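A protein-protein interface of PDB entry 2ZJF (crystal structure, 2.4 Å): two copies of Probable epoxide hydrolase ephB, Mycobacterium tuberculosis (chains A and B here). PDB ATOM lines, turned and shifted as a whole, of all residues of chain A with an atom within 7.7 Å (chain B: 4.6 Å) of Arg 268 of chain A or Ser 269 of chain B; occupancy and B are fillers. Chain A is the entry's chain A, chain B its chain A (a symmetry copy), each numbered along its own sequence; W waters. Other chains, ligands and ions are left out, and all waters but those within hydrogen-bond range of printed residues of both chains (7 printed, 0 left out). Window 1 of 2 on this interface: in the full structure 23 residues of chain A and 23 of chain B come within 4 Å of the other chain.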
ATOM      1  N   ARG A  20      24.934  16.518 -16.953  1.00  0.00           N
ATOM      2  CA  ARG A  20      26.061  15.787 -16.396  1.00  0.00           C
ATOM      3  C   ARG A  20      26.875  15.140 -17.500  1.00  0.00           C
ATOM      4  O   ARG A  20      26.342  14.393 -18.318  1.00  0.00           O
ATOM      5  CB  ARG A  20      25.570  14.702 -15.433  1.00  0.00           C
ATOM      6  CG  ARG A  20      26.676  14.060 -14.608  1.00  0.00           C
ATOM      7  CD  ARG A  20      26.180  12.854 -13.810  1.00  0.00           C
ATOM      8  NE  ARG A  20      25.674  11.801 -14.688  1.00  0.00           N
ATOM      9  CZ  ARG A  20      24.385  11.542 -14.894  1.00  0.00           C
ATOM     10  NH1 ARG A  20      23.450  12.255 -14.280  1.00  0.00           N
ATOM     11  NH2 ARG A  20      24.031  10.570 -15.720  1.00  0.00           N
ATOM     12  N   GLY A  70      23.582  10.438 -23.124  1.00  0.00           N
ATOM     13  CA  GLY A  70      22.930   9.203 -23.532  1.00  0.00           C
ATOM     14  C   GLY A  70      23.851   7.997 -23.412  1.00  0.00           C
ATOM     15  O   GLY A  70      23.395   6.858 -23.412  1.00  0.00           O
ATOM     16  N   GLY A  72      27.432   5.969 -21.508  1.00  0.00           N
ATOM     17  CA  GLY A  72      28.129   5.707 -20.257  1.00  0.00           C
ATOM     18  C   GLY A  72      27.550   6.238 -18.959  1.00  0.00           C
ATOM     19  O   GLY A  72      26.502   5.776 -18.490  1.00  0.00           O
ATOM     20  N   ARG A  73      28.241   7.205 -18.358  1.00  0.00           N
ATOM     21  CA  ARG A  73      27.784   7.770 -17.091  1.00  0.00           C
ATOM     22  C   ARG A  73      27.193   9.168 -17.237  1.00  0.00           C
ATOM     23  O   ARG A  73      26.846   9.803 -16.242  1.00  0.00           O
ATOM     24  CB  ARG A  73      28.933   7.800 -16.069  1.00  0.00           C
ATOM     25  CG  ARG A  73      29.489   6.429 -15.690  1.00  0.00           C
ATOM     26  CD  ARG A  73      30.639   6.567 -14.698  1.00  0.00           C
ATOM     27  NE  ARG A  73      30.228   7.270 -13.480  1.00  0.00           N
ATOM     28  CZ  ARG A  73      31.072   7.801 -12.592  1.00  0.00           C
ATOM     29  NH1 ARG A  73      32.389   7.716 -12.775  1.00  0.00           N
ATOM     30  NH2 ARG A  73      30.600   8.429 -11.523  1.00  0.00           N
ATOM     31  N   SER A  74      27.076   9.647 -18.473  1.00  0.00           N
ATOM     32  CA  SER A  74      26.521  10.979 -18.708  1.00  0.00           C
ATOM     33  C   SER A  74      24.996  10.950 -18.705  1.00  0.00           C
ATOM     34  O   SER A  74      24.395   9.898 -18.910  1.00  0.00           O
ATOM     35  CB  SER A  74      27.035  11.533 -20.029  1.00  0.00           C
ATOM     36  OG  SER A  74      28.441  11.635 -19.974  1.00  0.00           O
ATOM     37  N   SER A  75      24.386  12.109 -18.458  1.00  0.00           N
ATOM     38  CA  SER A  75      22.929  12.246 -18.402  1.00  0.00           C
ATOM     39  C   SER A  75      22.190  11.522 -19.517  1.00  0.00           C
ATOM     40  O   SER A  75      22.551  11.625 -20.695  1.00  0.00           O
ATOM     41  CB  SER A  75      22.533  13.722 -18.427  1.00  0.00           C
ATOM     42  OG  SER A  75      22.936  14.370 -17.240  1.00  0.00           O
ATOM     43  N   LYS A  76      21.145  10.799 -19.125  1.00  0.00           N
ATOM     44  CA  LYS A  76      20.324  10.035 -20.055  1.00  0.00           C
ATOM     45  C   LYS A  76      18.947  10.679 -20.204  1.00  0.00           C
ATOM     46  O   LYS A  76      18.086  10.511 -19.340  1.00  0.00           O
ATOM     47  CB  LYS A  76      20.146   8.597 -19.546  1.00  0.00           C
ATOM     48  CG  LYS A  76      21.437   7.848 -19.237  1.00  0.00           C
ATOM     49  CD  LYS A  76      22.351   7.787 -20.441  1.00  0.00           C
ATOM     50  CE  LYS A  76      23.510   6.847 -20.190  1.00  0.00           C
ATOM     51  NZ  LYS A  76      24.239   7.198 -18.953  1.00  0.00           N
ATOM     52  N   TYR A  77      18.740  11.417 -21.294  1.00  0.00           N
ATOM     53  CA  TYR A  77      17.449  12.071 -21.552  1.00  0.00           C
ATOM     54  C   TYR A  77      16.571  11.172 -22.409  1.00  0.00           C
ATOM     55  O   TYR A  77      17.080  10.428 -23.255  1.00  0.00           O
ATOM     56  CB  TYR A  77      17.652  13.384 -22.313  1.00  0.00           C
ATOM     57  CG  TYR A  77      18.370  14.451 -21.539  1.00  0.00           C
ATOM     58  CD1 TYR A  77      17.723  15.161 -20.529  1.00  0.00           C
ATOM     59  CD2 TYR A  77      19.709  14.731 -21.792  1.00  0.00           C
ATOM     60  CE1 TYR A  77      18.397  16.126 -19.788  1.00  0.00           C
ATOM     61  CE2 TYR A  77      20.395  15.692 -21.056  1.00  0.00           C
ATOM     62  CZ  TYR A  77      19.734  16.386 -20.054  1.00  0.00           C
ATOM     63  OH  TYR A  77      20.415  17.332 -19.324  1.00  0.00           O
ATOM     64  N   GLU A 185      18.841  -6.288 -27.484  1.00  0.00           N
ATOM     65  CA  GLU A 185      18.639  -6.865 -26.161  1.00  0.00           C
ATOM     66  C   GLU A 185      18.609  -8.389 -26.060  1.00  0.00           C
ATOM     67  O   GLU A 185      18.880  -8.938 -24.992  1.00  0.00           O
ATOM     68  CB  GLU A 185      17.373  -6.282 -25.530  1.00  0.00           C
ATOM     69  CG  GLU A 185      17.480  -4.798 -25.199  1.00  0.00           C
ATOM     70  CD  GLU A 185      18.679  -4.481 -24.310  1.00  0.00           C
ATOM     71  OE1 GLU A 185      19.025  -5.317 -23.448  1.00  0.00           O
ATOM     72  OE2 GLU A 185      19.267  -3.392 -24.463  1.00  0.00           O
ATOM     73  N   LEU A 188      23.031  -8.651 -26.335  1.00  0.00           N
ATOM     74  CA  LEU A 188      23.801  -7.426 -26.497  1.00  0.00           C
ATOM     75  C   LEU A 188      25.294  -7.646 -26.703  1.00  0.00           C
ATOM     76  O   LEU A 188      25.894  -7.012 -27.564  1.00  0.00           O
ATOM     77  CB  LEU A 188      23.548  -6.494 -25.295  1.00  0.00           C
ATOM     78  CG  LEU A 188      24.115  -5.063 -25.288  1.00  0.00           C
ATOM     79  CD1 LEU A 188      23.343  -4.206 -24.275  1.00  0.00           C
ATOM     80  CD2 LEU A 188      25.602  -5.080 -24.946  1.00  0.00           C
ATOM     81  N   TYR A 262      32.706  -2.576 -23.094  1.00  0.00           N
ATOM     82  CA  TYR A 262      31.626  -1.984 -23.870  1.00  0.00           C
ATOM     83  C   TYR A 262      30.288  -2.628 -23.507  1.00  0.00           C
ATOM     84  O   TYR A 262      29.289  -1.929 -23.344  1.00  0.00           O
ATOM     85  CB  TYR A 262      31.902  -2.134 -25.369  1.00  0.00           C
ATOM     86  CG  TYR A 262      33.005  -1.228 -25.891  1.00  0.00           C
ATOM     87  CD1 TYR A 262      32.810   0.152 -26.000  1.00  0.00           C
ATOM     88  CD2 TYR A 262      34.236  -1.750 -26.291  1.00  0.00           C
ATOM     89  CE1 TYR A 262      33.815   0.987 -26.495  1.00  0.00           C
ATOM     90  CE2 TYR A 262      35.247  -0.924 -26.792  1.00  0.00           C
ATOM     91  CZ  TYR A 262      35.027   0.442 -26.893  1.00  0.00           C
ATOM     92  OH  TYR A 262      35.999   1.254 -27.430  1.00  0.00           O
ATOM     93  N   THR A 263      30.278  -3.954 -23.376  1.00  0.00           N
ATOM     94  CA  THR A 263      29.068  -4.682 -23.016  1.00  0.00           C
ATOM     95  C   THR A 263      28.563  -4.159 -21.679  1.00  0.00           C
ATOM     96  O   THR A 263      27.366  -3.932 -21.495  1.00  0.00           O
ATOM     97  CB  THR A 263      29.335  -6.206 -22.876  1.00  0.00           C
ATOM     98  OG1 THR A 263      29.627  -6.761 -24.163  1.00  0.00           O
ATOM     99  CG2 THR A 263      28.114  -6.921 -22.292  1.00  0.00           C
ATOM    100  N   GLY A 264      29.491  -3.971 -20.747  1.00  0.00           N
ATOM    101  CA  GLY A 264      29.136  -3.468 -19.434  1.00  0.00           C
ATOM    102  C   GLY A 264      28.514  -2.087 -19.499  1.00  0.00           C
ATOM    103  O   GLY A 264      27.535  -1.809 -18.805  1.00  0.00           O
ATOM    104  N   GLU A 265      29.066  -1.220 -20.339  1.00  0.00           N
ATOM    105  CA  GLU A 265      28.544   0.137 -20.458  1.00  0.00           C
ATOM    106  C   GLU A 265      27.122   0.168 -21.001  1.00  0.00           C
ATOM    107  O   GLU A 265      26.243   0.841 -20.451  1.00  0.00           O
ATOM    108  CB  GLU A 265      29.437   0.985 -21.374  1.00  0.00           C
ATOM    109  CG  GLU A 265      30.861   1.187 -20.869  1.00  0.00           C
ATOM    110  CD  GLU A 265      30.913   1.988 -19.587  1.00  0.00           C
ATOM    111  OE1 GLU A 265      30.635   3.207 -19.635  1.00  0.00           O
ATOM    112  OE2 GLU A 265      31.227   1.398 -18.528  1.00  0.00           O
ATOM    113  N   PHE A 266      26.902  -0.571 -22.083  1.00  0.00           N
ATOM    114  CA  PHE A 266      25.602  -0.590 -22.735  1.00  0.00           C
ATOM    115  C   PHE A 266      24.467  -1.383 -22.083  1.00  0.00           C
ATOM    116  O   PHE A 266      23.299  -1.037 -22.269  1.00  0.00           O
ATOM    117  CB  PHE A 266      25.792  -0.995 -24.195  1.00  0.00           C
ATOM    118  CG  PHE A 266      26.429   0.082 -25.026  1.00  0.00           C
ATOM    119  CD1 PHE A 266      25.676   1.165 -25.477  1.00  0.00           C
ATOM    120  CD2 PHE A 266      27.792   0.051 -25.304  1.00  0.00           C
ATOM    121  CE1 PHE A 266      26.268   2.201 -26.188  1.00  0.00           C
ATOM    122  CE2 PHE A 266      28.395   1.088 -26.016  1.00  0.00           C
ATOM    123  CZ  PHE A 266      27.631   2.165 -26.457  1.00  0.00           C
ATOM    124  N   GLU A 267      24.762  -2.427 -21.319  1.00  0.00           N
ATOM    125  CA  GLU A 267      23.640  -3.112 -20.702  1.00  0.00           C
ATOM    126  C   GLU A 267      23.175  -2.318 -19.494  1.00  0.00           C
ATOM    127  O   GLU A 267      22.211  -2.680 -18.828  1.00  0.00           O
ATOM    128  CB  GLU A 267      23.970  -4.568 -20.342  1.00  0.00           C
ATOM    129  CG  GLU A 267      25.208  -4.816 -19.538  1.00  0.00           C
ATOM    130  CD  GLU A 267      25.447  -6.308 -19.351  1.00  0.00           C
ATOM    131  OE1 GLU A 267      25.285  -7.053 -20.343  1.00  0.00           O
ATOM    132  OE2 GLU A 267      25.794  -6.732 -18.226  1.00  0.00           O
ATOM    133  N   ARG A 268      23.861  -1.210 -19.243  1.00  0.00           N
ATOM    134  CA  ARG A 268      23.520  -0.313 -18.144  1.00  0.00           C
ATOM    135  C   ARG A 268      22.906   0.966 -18.715  1.00  0.00           C
ATOM    136  O   ARG A 268      21.948   1.512 -18.163  1.00  0.00           O
ATOM    137  CB  ARG A 268      24.766   0.056 -17.336  1.00  0.00           C
ATOM    138  CG  ARG A 268      25.252  -1.000 -16.346  1.00  0.00           C
ATOM    139  CD  ARG A 268      26.524  -0.521 -15.676  1.00  0.00           C
ATOM    140  NE  ARG A 268      26.924  -1.324 -14.528  1.00  0.00           N
ATOM    141  CZ  ARG A 268      26.241  -1.409 -13.387  1.00  0.00           C
ATOM    142  NH1 ARG A 268      25.103  -0.738 -13.232  1.00  0.00           N
ATOM    143  NH2 ARG A 268      26.706  -2.155 -12.388  1.00  0.00           N
ATOM    144  N   SER A 269      23.460   1.433 -19.830  1.00  0.00           N
ATOM    145  CA  SER A 269      22.988   2.661 -20.462  1.00  0.00           C
ATOM    146  C   SER A 269      21.855   2.431 -21.448  1.00  0.00           C
ATOM    147  O   SER A 269      20.953   3.261 -21.568  1.00  0.00           O
ATOM    148  CB  SER A 269      24.131   3.347 -21.213  1.00  0.00           C
ATOM    149  OG  SER A 269      24.357   2.715 -22.469  1.00  0.00           O
ATOM    150  N   GLY A 270      21.914   1.305 -22.155  1.00  0.00           N
ATOM    151  CA  GLY A 270      20.912   1.011 -23.160  1.00  0.00           C
ATOM    152  C   GLY A 270      21.313   1.739 -24.432  1.00  0.00           C
ATOM    153  O   GLY A 270      22.335   2.424 -24.447  1.00  0.00           O
ATOM    154  N   PHE A 271      20.521   1.601 -25.492  1.00  0.00           N
ATOM    155  CA  PHE A 271      20.819   2.258 -26.761  1.00  0.00           C
ATOM    156  C   PHE A 271      19.835   3.382 -27.092  1.00  0.00           C
ATOM    157  O   PHE A 271      19.955   4.024 -28.131  1.00  0.00           O
ATOM    158  CB  PHE A 271      20.815   1.227 -27.889  1.00  0.00           C
ATOM    159  CG  PHE A 271      22.000   0.314 -27.873  1.00  0.00           C
ATOM    160  CD1 PHE A 271      23.059   0.511 -28.754  1.00  0.00           C
ATOM    161  CD2 PHE A 271      22.074  -0.732 -26.959  1.00  0.00           C
ATOM    162  CE1 PHE A 271      24.179  -0.325 -28.724  1.00  0.00           C
ATOM    163  CE2 PHE A 271      23.188  -1.572 -26.918  1.00  0.00           C
ATOM    164  CZ  PHE A 271      24.240  -1.372 -27.797  1.00  0.00           C
ATOM    165  N   GLY B  70      14.734  -1.880 -17.507  1.00  0.00           N
ATOM    166  CA  GLY B  70      14.872  -0.434 -17.443  1.00  0.00           C
ATOM    167  C   GLY B  70      15.802   0.009 -16.322  1.00  0.00           C
ATOM    168  O   GLY B  70      16.274   1.141 -16.310  1.00  0.00           O
ATOM    169  N   GLY B  72      19.251  -0.863 -13.512  1.00  0.00           N
ATOM    170  CA  GLY B  72      20.585  -1.438 -13.402  1.00  0.00           C
ATOM    171  C   GLY B  72      21.253  -2.006 -14.640  1.00  0.00           C
ATOM    172  O   GLY B  72      21.631  -1.268 -15.559  1.00  0.00           O
ATOM    173  N   ARG B  73      21.421  -3.327 -14.665  1.00  0.00           N
ATOM    174  CA  ARG B  73      22.074  -3.973 -15.801  1.00  0.00           C
ATOM    175  C   ARG B  73      21.103  -4.727 -16.703  1.00  0.00           C
ATOM    176  O   ARG B  73      21.521  -5.392 -17.649  1.00  0.00           O
ATOM    177  CB  ARG B  73      23.175  -4.931 -15.315  1.00  0.00           C
ATOM    178  CG  ARG B  73      24.317  -4.262 -14.554  1.00  0.00           C
ATOM    179  CD  ARG B  73      25.338  -5.295 -14.090  1.00  0.00           C
ATOM    180  NE  ARG B  73      25.892  -6.057 -15.212  1.00  0.00           N
ATOM    181  CZ  ARG B  73      26.555  -7.209 -15.091  1.00  0.00           C
ATOM    182  NH1 ARG B  73      26.756  -7.751 -13.890  1.00  0.00           N
ATOM    183  NH2 ARG B  73      27.010  -7.830 -16.171  1.00  0.00           N
ATOM    184  N   LYS B  76      17.289  -2.289 -21.427  1.00  0.00           N
ATOM    185  CA  LYS B  76      16.715  -0.951 -21.432  1.00  0.00           C
ATOM    186  C   LYS B  76      15.940  -0.707 -22.725  1.00  0.00           C
ATOM    187  O   LYS B  76      16.539  -0.431 -23.765  1.00  0.00           O
ATOM    188  CB  LYS B  76      17.827   0.102 -21.314  1.00  0.00           C
ATOM    189  CG  LYS B  76      18.768  -0.070 -20.127  1.00  0.00           C
ATOM    190  CD  LYS B  76      18.016  -0.076 -18.814  1.00  0.00           C
ATOM    191  CE  LYS B  76      18.975  -0.009 -17.644  1.00  0.00           C
ATOM    192  NZ  LYS B  76      19.992  -1.080 -17.712  1.00  0.00           N
ATOM    193  N   GLU B 265      24.265   3.583 -10.224  1.00  0.00           N
ATOM    194  CA  GLU B 265      23.353   2.818 -11.067  1.00  0.00           C
ATOM    195  C   GLU B 265      22.553   3.703 -12.012  1.00  0.00           C
ATOM    196  O   GLU B 265      22.461   3.432 -13.215  1.00  0.00           O
ATOM    197  CB  GLU B 265      22.373   2.007 -10.208  1.00  0.00           C
ATOM    198  CG  GLU B 265      23.022   0.949  -9.324  1.00  0.00           C
ATOM    199  CD  GLU B 265      23.687  -0.148 -10.125  1.00  0.00           C
ATOM    200  OE1 GLU B 265      22.962  -0.953 -10.749  1.00  0.00           O
ATOM    201  OE2 GLU B 265      24.938  -0.204 -10.134  1.00  0.00           O
ATOM    202  N   PHE B 266      21.983   4.769 -11.461  1.00  0.00           N
ATOM    203  CA  PHE B 266      21.148   5.669 -12.241  1.00  0.00           C
ATOM    204  C   PHE B 266      21.825   6.650 -13.199  1.00  0.00           C
ATOM    205  O   PHE B 266      21.220   7.036 -14.201  1.00  0.00           O
ATOM    206  CB  PHE B 266      20.189   6.391 -11.295  1.00  0.00           C
ATOM    207  CG  PHE B 266      19.103   5.499 -10.766  1.00  0.00           C
ATOM    208  CD1 PHE B 266      18.001   5.181 -11.559  1.00  0.00           C
ATOM    209  CD2 PHE B 266      19.208   4.924  -9.503  1.00  0.00           C
ATOM    210  CE1 PHE B 266      17.023   4.304 -11.106  1.00  0.00           C
ATOM    211  CE2 PHE B 266      18.232   4.041  -9.041  1.00  0.00           C
ATOM    212  CZ  PHE B 266      17.139   3.730  -9.846  1.00  0.00           C
ATOM    213  N   GLU B 267      23.058   7.064 -12.939  1.00  0.00           N
ATOM    214  CA  GLU B 267      23.654   7.966 -13.908  1.00  0.00           C
ATOM    215  C   GLU B 267      24.141   7.163 -15.101  1.00  0.00           C
ATOM    216  O   GLU B 267      24.651   7.712 -16.072  1.00  0.00           O
ATOM    217  CB  GLU B 267      24.772   8.825 -13.298  1.00  0.00           C
ATOM    218  CG  GLU B 267      25.854   8.116 -12.545  1.00  0.00           C
ATOM    219  CD  GLU B 267      26.825   9.109 -11.922  1.00  0.00           C
ATOM    220  OE1 GLU B 267      26.345  10.118 -11.360  1.00  0.00           O
ATOM    221  OE2 GLU B 267      28.054   8.883 -11.989  1.00  0.00           O
ATOM    222  N   ARG B 268      23.946   5.852 -15.024  1.00  0.00           N
ATOM    223  CA  ARG B 268      24.318   4.943 -16.101  1.00  0.00           C
ATOM    224  C   ARG B 268      23.050   4.440 -16.792  1.00  0.00           C
ATOM    225  O   ARG B 268      23.004   4.308 -18.018  1.00  0.00           O
ATOM    226  CB  ARG B 268      25.092   3.740 -15.555  1.00  0.00           C
ATOM    227  CG  ARG B 268      26.564   3.989 -15.233  1.00  0.00           C
ATOM    228  CD  ARG B 268      27.173   2.734 -14.642  1.00  0.00           C
ATOM    229  NE  ARG B 268      28.626   2.772 -14.546  1.00  0.00           N
ATOM    230  CZ  ARG B 268      29.454   2.797 -15.591  1.00  0.00           C
ATOM    231  NH1 ARG B 268      28.973   2.795 -16.831  1.00  0.00           N
ATOM    232  NH2 ARG B 268      30.770   2.809 -15.395  1.00  0.00           N
ATOM    233  N   SER B 269      22.019   4.169 -15.997  1.00  0.00           N
ATOM    234  CA  SER B 269      20.759   3.656 -16.527  1.00  0.00           C
ATOM    235  C   SER B 269      19.794   4.752 -16.947  1.00  0.00           C
ATOM    236  O   SER B 269      19.060   4.596 -17.924  1.00  0.00           O
ATOM    237  CB  SER B 269      20.058   2.788 -15.481  1.00  0.00           C
ATOM    238  OG  SER B 269      19.392   3.601 -14.520  1.00  0.00           O
ATOM    239  N   GLY B 270      19.796   5.853 -16.199  1.00  0.00           N
ATOM    240  CA  GLY B 270      18.879   6.938 -16.482  1.00  0.00           C
ATOM    241  C   GLY B 270      17.550   6.594 -15.832  1.00  0.00           C
ATOM    242  O   GLY B 270      17.428   5.537 -15.213  1.00  0.00           O
ATOM    243  N   PHE B 271      16.556   7.468 -15.969  1.00  0.00           N
ATOM    244  CA  PHE B 271      15.241   7.231 -15.381  1.00  0.00           C
ATOM    245  C   PHE B 271      14.164   6.957 -16.434  1.00  0.00           C
ATOM    246  O   PHE B 271      13.004   6.743 -16.091  1.00  0.00           O
ATOM    247  CB  PHE B 271      14.831   8.432 -14.532  1.00  0.00           C
ATOM    248  CG  PHE B 271      15.588   8.545 -13.246  1.00  0.00           C
ATOM    249  CD1 PHE B 271      15.006   8.150 -12.044  1.00  0.00           C
ATOM    250  CD2 PHE B 271      16.895   9.021 -13.233  1.00  0.00           C
ATOM    251  CE1 PHE B 271      15.720   8.229 -10.845  1.00  0.00           C
ATOM    252  CE2 PHE B 271      17.618   9.103 -12.042  1.00  0.00           C
ATOM    253  CZ  PHE B 271      17.035   8.709 -10.849  1.00  0.00           C
HETATM  254  O   HOH W   1      18.621  -0.880 -25.307  1.00  0.00           O
HETATM  255  O   HOH W   2      16.536   7.596 -19.380  1.00  0.00           O
HETATM  256  O   HOH W   3      21.657   9.450 -15.616  1.00  0.00           O
HETATM  257  O   HOH W   4      17.627   2.675 -24.034  1.00  0.00           O
HETATM  258  O   HOH W   5      22.978   0.839 -14.475  1.00  0.00           O
HETATM  259  O   HOH W   6      26.642   3.056 -18.575  1.00  0.00           O
HETATM  260  O   HOH W   7      17.527  10.332 -16.777  1.00  0.00           O
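O of Gly 72 of chain B is in hydrogen-bond range of NZ of Lys 76 of chain B, 2.7 Å away. O of Glu 265 of chain B sits at hydrogen-bond distance from OG of Ser 269 of chain B (3.3 Å). The guanidinium group of Arg 20 of chain A sits close to the backbone carbonyl oxygen of Ser 74 of chain A (3.3 Å). The side-chain amino group (NZ) of Lys 76 of chain A lies within hydrogen-bond range of the backbone carbonyl oxygen (O) of Ser 74 of chain A (2.7 Å). O of Glu 265 of chain A lies within hydrogen-bond range of OG of Ser 269 of chain A (3.3 Å). NZ of Lys 76 of chain A is in hydrogen-bond range of O of Gly 72 of chain A.
Of the printed residues of chain B, Lys 76 of chain A touches Glu 267, Arg 268 and Gly 270. Printed residues of chain B within 4 Å of Ser 269 of chain A: Arg 268. Of the printed residues of chain A, Glu 265 of chain B touches Arg 268 (3.1 Å). Of chain A, only Arg 268 comes within 4 Å of Ser 269 of chain B. Phe 271 of chain B touches none of the printed residues of chain A. The nearest printed residue of chain B that does not touch Arg 268 of chain A is Gly 270 of chain B (5.2 Å). The nearest residue of chain A that does not touch Ser 269 of chain B is Lys 76 of chain A (4.2 Å). The nearest printed residue of chain B that does not touch Lys 76 of chain A is Ser 269 of chain B (4.2 Å).
Of the 20 printed residues of chain A, 11 touch a printed residue of chain B. Of the 11 printed residues of chain B, 8 touch a printed residue of chain A. Among the printed residues, 22 pairs touch across the chains. Among the printed residues, Asp or Glu carboxylates within 4 Å of a Lys or Arg side-chain nitrogen of the other chain: Arg 20 of chain A with Glu 267 of chain B (3.8 Å), Arg 73 of chain A with Glu 267 of chain B (2.6 Å), Glu 265 of chain A with Arg 268 of chain B (3.1 Å), Glu 267 of chain A with Arg 73 of chain B (2.6 Å) and Arg 268 of chain A with Glu 265 of chain B (3.1 Å).
Gly 72 of chain A touches Arg 268 of chain B, and with the chains exchanged Arg 268 of chain A touches Gly 72 of chain B. Lys 76 of chain A touches Gly 270 of chain B, and with the chains exchanged Gly 270 of chain A touches Lys 76 of chain B. Glu 265 of chain A touches Arg 268 of chain B, and with the chains exchanged Arg 268 of chain A touches Glu 265 of chain B. Arg 268 of chain B touches its own counterpart, Arg 268 of chain A. Of the 22 pairs that touch across the chains among the printed residues, 19 have their exchanged pair printed and touching as well.
The backbone carbonyl oxygen (O) of Arg 268 of chain B sits close to the backbone carbonyl oxygen (O) of Arg 268 of chain A. The side-chain carboxylate of Glu 267 of chain B is in salt-bridge range of the guanidinium group of Arg 20 of chain A (3.8 Å). The backbone carbonyl oxygen of Arg 268 of chain A is in hydrogen-bond range of the side-chain amino group of Lys 76 of chain B (3.3 Å). The backbone carbonyl oxygen (O) of Arg 268 of chain A sits close to the backbone NH (N) of Ser 269 of chain B (3.4 Å). The side-chain carboxylate (OE2) of Glu 265 of chain A lies within salt-bridge range of the guanidinium group (NH1) of Arg 268 of chain B, 3.1 Å away. N of Ser 269 of chain A sits close to O of Arg 268 of chain B, 3.4 Å away. NH1 of Arg 268 of chain A lies within salt-bridge range of OE2 of Glu 265 of chain B (3.1 Å). NZ of Lys 76 of chain A is in hydrogen-bond range of O of Arg 268 of chain B. The side-chain carboxylate (OE2) of Glu 267 of chain B is in salt-bridge range of the guanidinium group (NH2) of Arg 73 of chain A (2.6 Å). OE2 of Glu 267 of chain A is in salt-bridge range of NH2 of Arg 73 of chain B (2.6 Å). The backbone carbonyl oxygen (O) of Glu 267 of chain A sits at hydrogen-bond distance from the side-chain amino group (NZ) of Lys 76 of chain B (3.0 Å). NZ of Lys 76 of chain A lies within hydrogen-bond range of O of Glu 267 of chain B (3.0 Å).
Among the printed residues, pairs that only touch across the chains: Gly 72 of chain A with Glu 267 of chain B, Gly 72 of chain A with Arg 268 of chain B, Arg 73 of chain A with Arg 268 of chain B, Ser 74 of chain A with Glu 267 of chain B, Lys 76 of chain A with Gly 270 of chain B, Glu 185 of chain A with Lys 76 of chain B, Glu 267 of chain A with Gly 72 of chain B, Arg 268 of chain A with Gly 72 of chain B, Arg 268 of chain A with Arg 73 of chain B and Gly 270 of chain A with Lys 76 of chain B.
Water W3 lies within hydrogen-bond range of NH2 of Arg 20 of chain A (2.6 Å), O of Phe 266 of chain B (2.8 Å) and O of Glu 267 of chain B (3.5 Å). Water W1 lies within hydrogen-bond range of O of Lys 76 of chain B, OE2 of Glu 185 of chain A and N of Phe 271 of chain A. Water W7 bridges the backbone carbonyl oxygen of Lys 76 of chain A and the backbone NH of Phe 271 of chain B. Water W6 lies within hydrogen-bond range of the backbone carbonyl oxygen of Gly 72 of chain A (2.7 Å), the guanidinium group of Arg 268 of chain B (2.9 Å) and the backbone carbonyl oxygen of Glu 265 of chain A (2.9 Å). Water W4 lies within hydrogen-bond range of O of Lys 76 of chain B and N of Phe 271 of chain A. Water W2 bridges the backbone carbonyl oxygen of Lys 76 of chain A (3.3 Å) and the backbone NH of Phe 271 of chain B (3.4 Å).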
